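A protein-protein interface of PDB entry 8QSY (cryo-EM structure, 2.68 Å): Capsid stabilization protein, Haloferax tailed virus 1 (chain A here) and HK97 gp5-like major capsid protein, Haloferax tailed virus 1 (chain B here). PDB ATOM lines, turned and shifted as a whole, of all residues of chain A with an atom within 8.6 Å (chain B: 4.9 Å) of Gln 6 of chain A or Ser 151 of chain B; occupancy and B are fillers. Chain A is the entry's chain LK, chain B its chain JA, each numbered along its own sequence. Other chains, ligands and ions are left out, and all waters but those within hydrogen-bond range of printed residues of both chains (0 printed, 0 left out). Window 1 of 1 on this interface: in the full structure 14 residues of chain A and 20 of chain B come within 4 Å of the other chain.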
ATOM      1  N   THR A   3     -34.556  31.403 -12.769  1.00  0.00           N
ATOM      2  CA  THR A   3     -33.569  31.416 -13.848  1.00  0.00           C
ATOM      3  C   THR A   3     -32.125  31.299 -13.344  1.00  0.00           C
ATOM      4  O   THR A   3     -31.697  32.079 -12.494  1.00  0.00           O
ATOM      5  CB  THR A   3     -33.751  32.709 -14.657  1.00  0.00           C
ATOM      6  OG1 THR A   3     -34.984  32.617 -15.366  1.00  0.00           O
ATOM      7  CG2 THR A   3     -32.645  33.025 -15.644  1.00  0.00           C
ATOM      8  N   GLU A   4     -31.337  30.376 -13.932  1.00  0.00           N
ATOM      9  CA  GLU A   4     -29.876  30.435 -13.898  1.00  0.00           C
ATOM     10  C   GLU A   4     -29.380  31.385 -14.996  1.00  0.00           C
ATOM     11  O   GLU A   4     -29.939  31.424 -16.092  1.00  0.00           O
ATOM     12  CB  GLU A   4     -29.242  29.069 -14.198  1.00  0.00           C
ATOM     13  CG  GLU A   4     -29.358  28.001 -13.106  1.00  0.00           C
ATOM     14  CD  GLU A   4     -28.369  26.841 -13.221  1.00  0.00           C
ATOM     15  OE1 GLU A   4     -27.231  27.080 -13.680  1.00  0.00           O
ATOM     16  OE2 GLU A   4     -28.730  25.699 -12.830  1.00  0.00           O
ATOM     17  N   THR A   5     -28.273  32.104 -14.742  1.00  0.00           N
ATOM     18  CA  THR A   5     -27.577  32.846 -15.793  1.00  0.00           C
ATOM     19  C   THR A   5     -26.229  32.187 -16.087  1.00  0.00           C
ATOM     20  O   THR A   5     -25.470  31.887 -15.168  1.00  0.00           O
ATOM     21  CB  THR A   5     -27.370  34.320 -15.422  1.00  0.00           C
ATOM     22  OG1 THR A   5     -28.629  34.895 -15.077  1.00  0.00           O
ATOM     23  CG2 THR A   5     -26.780  35.138 -16.545  1.00  0.00           C
ATOM     24  N   GLN A   6     -25.928  31.977 -17.377  1.00  0.00           N
ATOM     25  CA  GLN A   6     -24.701  31.332 -17.828  1.00  0.00           C
ATOM     26  C   GLN A   6     -24.169  32.083 -19.054  1.00  0.00           C
ATOM     27  O   GLN A   6     -24.537  31.768 -20.185  1.00  0.00           O
ATOM     28  CB  GLN A   6     -24.952  29.845 -18.125  1.00  0.00           C
ATOM     29  CG  GLN A   6     -25.394  29.012 -16.921  1.00  0.00           C
ATOM     30  CD  GLN A   6     -25.630  27.547 -17.210  1.00  0.00           C
ATOM     31  OE1 GLN A   6     -25.477  27.080 -18.337  1.00  0.00           O
ATOM     32  NE2 GLN A   6     -26.012  26.798 -16.187  1.00  0.00           N
ATOM     33  N   GLY A   7     -23.345  33.119 -18.835  1.00  0.00           N
ATOM     34  CA  GLY A   7     -22.897  33.993 -19.914  1.00  0.00           C
ATOM     35  C   GLY A   7     -24.025  34.883 -20.433  1.00  0.00           C
ATOM     36  O   GLY A   7     -24.671  35.577 -19.656  1.00  0.00           O
ATOM     37  N   GLU A   8     -24.254  34.878 -21.754  1.00  0.00           N
ATOM     38  CA  GLU A   8     -25.381  35.587 -22.358  1.00  0.00           C
ATOM     39  C   GLU A   8     -26.725  34.977 -21.936  1.00  0.00           C
ATOM     40  O   GLU A   8     -27.762  35.650 -21.951  1.00  0.00           O
ATOM     41  CB  GLU A   8     -25.352  35.523 -23.891  1.00  0.00           C
ATOM     42  CG  GLU A   8     -23.982  35.533 -24.552  1.00  0.00           C
ATOM     43  CD  GLU A   8     -23.368  34.154 -24.728  1.00  0.00           C
ATOM     44  OE1 GLU A   8     -22.609  33.738 -23.822  1.00  0.00           O
ATOM     45  OE2 GLU A   8     -23.591  33.542 -25.791  1.00  0.00           O
ATOM     46  N   HIS A   9     -26.701  33.682 -21.605  1.00  0.00           N
ATOM     47  CA  HIS A   9     -27.881  32.839 -21.595  1.00  0.00           C
ATOM     48  C   HIS A   9     -28.598  32.871 -20.247  1.00  0.00           C
ATOM     49  O   HIS A   9     -27.984  32.788 -19.179  1.00  0.00           O
ATOM     50  CB  HIS A   9     -27.480  31.404 -21.918  1.00  0.00           C
ATOM     51  CG  HIS A   9     -26.717  31.249 -23.186  1.00  0.00           C
ATOM     52  ND1 HIS A   9     -27.186  31.674 -24.417  1.00  0.00           N
ATOM     53  CD2 HIS A   9     -25.511  30.697 -23.402  1.00  0.00           C
ATOM     54  CE1 HIS A   9     -26.288  31.392 -25.341  1.00  0.00           C
ATOM     55  NE2 HIS A   9     -25.260  30.779 -24.742  1.00  0.00           N
ATOM     56  N   THR A  10     -29.931  32.894 -20.325  1.00  0.00           N
ATOM     57  CA  THR A  10     -30.793  32.588 -19.193  1.00  0.00           C
ATOM     58  C   THR A  10     -31.399  31.205 -19.402  1.00  0.00           C
ATOM     59  O   THR A  10     -32.010  30.943 -20.437  1.00  0.00           O
ATOM     60  CB  THR A  10     -31.889  33.645 -19.032  1.00  0.00           C
ATOM     61  OG1 THR A  10     -32.580  33.800 -20.272  1.00  0.00           O
ATOM     62  CG2 THR A  10     -31.333  34.980 -18.595  1.00  0.00           C
ATOM     63  N   PHE A  11     -31.238  30.327 -18.405  1.00  0.00           N
ATOM     64  CA  PHE A  11     -31.820  28.995 -18.422  1.00  0.00           C
ATOM     65  C   PHE A  11     -32.900  28.887 -17.352  1.00  0.00           C
ATOM     66  O   PHE A  11     -32.650  29.211 -16.196  1.00  0.00           O
ATOM     67  CB  PHE A  11     -30.739  27.951 -18.148  1.00  0.00           C
ATOM     68  CG  PHE A  11     -29.801  27.720 -19.302  1.00  0.00           C
ATOM     69  CD1 PHE A  11     -28.634  28.462 -19.431  1.00  0.00           C
ATOM     70  CD2 PHE A  11     -30.090  26.757 -20.262  1.00  0.00           C
ATOM     71  CE1 PHE A  11     -27.772  28.232 -20.495  1.00  0.00           C
ATOM     72  CE2 PHE A  11     -29.232  26.539 -21.331  1.00  0.00           C
ATOM     73  CZ  PHE A  11     -28.074  27.278 -21.445  1.00  0.00           C
ATOM     74  N   PRO A  12     -34.123  28.415 -17.683  1.00  0.00           N
ATOM     75  CA  PRO A  12     -35.123  28.116 -16.658  1.00  0.00           C
ATOM     76  C   PRO A  12     -34.640  26.973 -15.766  1.00  0.00           C
ATOM     77  O   PRO A  12     -34.060  25.996 -16.244  1.00  0.00           O
ATOM     78  CB  PRO A  12     -36.346  27.672 -17.478  1.00  0.00           C
ATOM     79  CG  PRO A  12     -36.130  28.290 -18.848  1.00  0.00           C
ATOM     80  CD  PRO A  12     -34.634  28.186 -19.044  1.00  0.00           C
ATOM     81  N   VAL A  13     -34.885  27.090 -14.456  1.00  0.00           N
ATOM     82  CA  VAL A  13     -34.549  26.017 -13.520  1.00  0.00           C
ATOM     83  C   VAL A  13     -35.560  24.874 -13.633  1.00  0.00           C
ATOM     84  O   VAL A  13     -36.753  25.099 -13.820  1.00  0.00           O
ATOM     85  CB  VAL A  13     -34.400  26.504 -12.063  1.00  0.00           C
ATOM     86  CG1 VAL A  13     -33.408  27.645 -11.957  1.00  0.00           C
ATOM     87  CG2 VAL A  13     -35.725  26.893 -11.426  1.00  0.00           C
ATOM     88  N   ILE B 149     -29.343  25.718 -27.230  1.00  0.00           N
ATOM     89  CA  ILE B 149     -28.128  25.747 -26.433  1.00  0.00           C
ATOM     90  C   ILE B 149     -28.361  24.889 -25.193  1.00  0.00           C
ATOM     91  O   ILE B 149     -29.317  25.115 -24.459  1.00  0.00           O
ATOM     92  CB  ILE B 149     -27.769  27.192 -26.022  1.00  0.00           C
ATOM     93  CG1 ILE B 149     -27.884  28.229 -27.147  1.00  0.00           C
ATOM     94  CG2 ILE B 149     -26.408  27.230 -25.347  1.00  0.00           C
ATOM     95  CD1 ILE B 149     -27.009  27.974 -28.363  1.00  0.00           C
ATOM     96  N   ALA B 150     -27.474  23.921 -24.953  1.00  0.00           N
ATOM     97  CA  ALA B 150     -27.487  23.149 -23.720  1.00  0.00           C
ATOM     98  C   ALA B 150     -26.845  23.938 -22.577  1.00  0.00           C
ATOM     99  O   ALA B 150     -25.889  24.684 -22.776  1.00  0.00           O
ATOM    100  CB  ALA B 150     -26.778  21.841 -23.949  1.00  0.00           C
ATOM    101  N   SER B 151     -27.362  23.735 -21.362  1.00  0.00           N
ATOM    102  CA  SER B 151     -26.765  24.278 -20.146  1.00  0.00           C
ATOM    103  C   SER B 151     -25.385  23.678 -19.869  1.00  0.00           C
ATOM    104  O   SER B 151     -25.073  22.562 -20.291  1.00  0.00           O
ATOM    105  CB  SER B 151     -27.681  24.105 -18.966  1.00  0.00           C
ATOM    106  OG  SER B 151     -28.311  22.832 -19.012  1.00  0.00           O
ATOM    107  N   ASP B 152     -24.578  24.426 -19.111  1.00  0.00           N
ATOM    108  CA  ASP B 152     -23.235  24.026 -18.711  1.00  0.00           C
ATOM    109  C   ASP B 152     -23.205  22.696 -17.949  1.00  0.00           C
ATOM    110  O   ASP B 152     -24.179  22.297 -17.309  1.00  0.00           O
ATOM    111  CB  ASP B 152     -22.608  25.091 -17.811  1.00  0.00           C
ATOM    112  CG  ASP B 152     -22.352  26.436 -18.475  1.00  0.00           C
ATOM    113  OD1 ASP B 152     -22.338  26.500 -19.724  1.00  0.00           O
ATOM    114  OD2 ASP B 152     -22.153  27.427 -17.741  1.00  0.00           O
ATOM    115  N   GLU B 153     -22.039  22.034 -17.982  1.00  0.00           N
ATOM    116  CA  GLU B 153     -21.739  20.953 -17.054  1.00  0.00           C
ATOM    117  C   GLU B 153     -21.818  21.446 -15.604  1.00  0.00           C
ATOM    118  O   GLU B 153     -21.282  22.506 -15.256  1.00  0.00           O
ATOM    119  CB  GLU B 153     -20.350  20.382 -17.340  1.00  0.00           C
ATOM    120  CG  GLU B 153     -20.290  19.465 -18.548  1.00  0.00           C
ATOM    121  CD  GLU B 153     -18.924  18.853 -18.817  1.00  0.00           C
ATOM    122  OE1 GLU B 153     -17.977  19.106 -18.035  1.00  0.00           O
ATOM    123  OE2 GLU B 153     -18.807  18.121 -19.815  1.00  0.00           O
ATOM    124  N   GLU B 170     -30.540  17.955 -17.884  1.00  0.00           N
ATOM    125  CA  GLU B 170     -30.116  18.995 -18.813  1.00  0.00           C
ATOM    126  C   GLU B 170     -31.285  19.932 -19.129  1.00  0.00           C
ATOM    127  O   GLU B 170     -32.392  19.475 -19.395  1.00  0.00           O
ATOM    128  CB  GLU B 170     -29.536  18.394 -20.094  1.00  0.00           C
ATOM    129  CG  GLU B 170     -28.603  19.351 -20.814  1.00  0.00           C
ATOM    130  CD  GLU B 170     -27.799  18.713 -21.936  1.00  0.00           C
ATOM    131  OE1 GLU B 170     -28.411  18.084 -22.823  1.00  0.00           O
ATOM    132  OE2 GLU B 170     -26.556  18.851 -21.926  1.00  0.00           O
ATOM    133  N   THR B 171     -31.023  21.245 -19.092  1.00  0.00           N
ATOM    134  CA  THR B 171     -32.001  22.276 -19.419  1.00  0.00           C
ATOM    135  C   THR B 171     -31.481  23.092 -20.604  1.00  0.00           C
ATOM    136  O   THR B 171     -30.274  23.225 -20.766  1.00  0.00           O
ATOM    137  CB  THR B 171     -32.345  23.098 -18.169  1.00  0.00           C
ATOM    138  OG1 THR B 171     -33.319  24.075 -18.527  1.00  0.00           O
ATOM    139  CG2 THR B 171     -31.163  23.809 -17.543  1.00  0.00           C
ATOM    140  N   TYR B 172     -32.395  23.607 -21.443  1.00  0.00           N
ATOM    141  CA  TYR B 172     -32.040  24.235 -22.710  1.00  0.00           C
ATOM    142  C   TYR B 172     -32.592  25.654 -22.815  1.00  0.00           C
ATOM    143  O   TYR B 172     -33.614  25.995 -22.226  1.00  0.00           O
ATOM    144  CB  TYR B 172     -32.533  23.397 -23.894  1.00  0.00           C
ATOM    145  CG  TYR B 172     -32.085  21.961 -23.830  1.00  0.00           C
ATOM    146  CD1 TYR B 172     -30.864  21.556 -24.358  1.00  0.00           C
ATOM    147  CD2 TYR B 172     -32.870  21.008 -23.194  1.00  0.00           C
ATOM    148  CE1 TYR B 172     -30.450  20.233 -24.266  1.00  0.00           C
ATOM    149  CE2 TYR B 172     -32.465  19.688 -23.085  1.00  0.00           C
ATOM    150  CZ  TYR B 172     -31.261  19.295 -23.643  1.00  0.00           C
ATOM    151  OH  TYR B 172     -30.862  17.995 -23.529  1.00  0.00           O
ATOM    152  N   ARG B 389     -19.086  33.486 -24.192  1.00  0.00           N
ATOM    153  CA  ARG B 389     -18.003  33.239 -23.242  1.00  0.00           C
ATOM    154  C   ARG B 389     -16.761  32.654 -23.912  1.00  0.00           C
ATOM    155  O   ARG B 389     -15.656  32.840 -23.416  1.00  0.00           O
ATOM    156  CB  ARG B 389     -18.455  32.311 -22.115  1.00  0.00           C
ATOM    157  CG  ARG B 389     -19.379  32.966 -21.101  1.00  0.00           C
ATOM    158  CD  ARG B 389     -19.991  31.968 -20.134  1.00  0.00           C
ATOM    159  NE  ARG B 389     -20.840  30.973 -20.778  1.00  0.00           N
ATOM    160  CZ  ARG B 389     -21.253  29.844 -20.211  1.00  0.00           C
ATOM    161  NH1 ARG B 389     -21.995  28.995 -20.901  1.00  0.00           N
ATOM    162  NH2 ARG B 389     -20.889  29.527 -18.980  1.00  0.00           N
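The side-chain amide oxygen (OE1) of Gln 6 of chain A sits at hydrogen-bond distance from the backbone NH (N) of Asp 152 of chain B (2.9 Å).
OG1 of Thr 171 of chain B is in hydrogen-bond range of O of Pro 12 of chain A.
The backbone carbonyl oxygen (O) of Thr 171 of chain B is in hydrogen-bond range of the side-chain hydroxyl (OG) of Ser 151 of chain B (2.7 Å).
The side-chain carboxylate (OD2) of Asp 152 of chain B is in salt-bridge range of the guanidinium group (NH2) of Arg 389 of chain B, at 2.7 Å.
The side-chain carboxylate of Glu 170 of chain B is in hydrogen-bond range of the side-chain hydroxyl of Tyr 172 of chain B (2.6 Å).
The side-chain carboxylate (OE1) of Glu 4 of chain A lies within hydrogen-bond range of the side-chain amide nitrogen (NE2) of Gln 6 of chain A (2.8 Å).
N of Glu 4 of chain A is in hydrogen-bond range of O of Phe 11 of chain A (2.9 Å).
The side-chain carboxylate of Glu 8 of chain A is in hydrogen-bond range of a ring nitrogen (NE2) of His 9 of chain A (3.4 Å).
Among the printed residues, merely in contact across the chains: Gln 6 of chain A with Ser 151 of chain B, Gln 6 of chain A with Arg 389 of chain B, Gly 7 of chain A with Arg 389 of chain B, Glu 8 of chain A with Arg 389 of chain B, His 9 of chain A with Ile 149 of chain B, Phe 11 of chain A with Ile 149 of chain B, Phe 11 of chain A with Ala 150 of chain B, Phe 11 of chain A with Ser 151 of chain B, Phe 11 of chain A with Thr 171 of chain B, Phe 11 of chain A with Tyr 172 of chain B and Pro 12 of chain A with Tyr 172 of chain B.
Of chain B, only Ser 151, Asp 152 and Arg 389 come within 4 Å of Gln 6 of chain A.
Of chain A, only Gln 6 (2.9 Å) comes within 4 Å of Asp 152 of chain B.
Of the printed residues of chain B, Phe 11 of chain A touches Ile 149 (3.4 Å), Ala 150 (3.6 Å), Ser 151 (3.4 Å), Thr 171 (3.5 Å) and Tyr 172 (3.7 Å).
Of the printed residues of chain A, Ile 149 of chain B touches His 9 and Phe 11.
Of the printed residues of chain B, Pro 12 of chain A touches Thr 171 (3.1 Å) and Tyr 172 (3.996 Å).
The nearest printed residue of chain B that does not touch Gln 6 of chain A is Ala 150 of chain B (5.1 Å).
The nearest residue of chain A that does not touch Ser 151 of chain B is Glu 4 of chain A (6.1 Å).
Of the 11 printed residues of chain A, 6 touch a printed residue of chain B.
Hydrophobic or aromatic side chains of chain A that line the printed part of chain B: His 9, Phe 11 and Pro 12.
Among the printed residues, no Asp or Glu carboxylate lies within 4 Å of a Lys or Arg side-chain nitrogen of the other chain.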
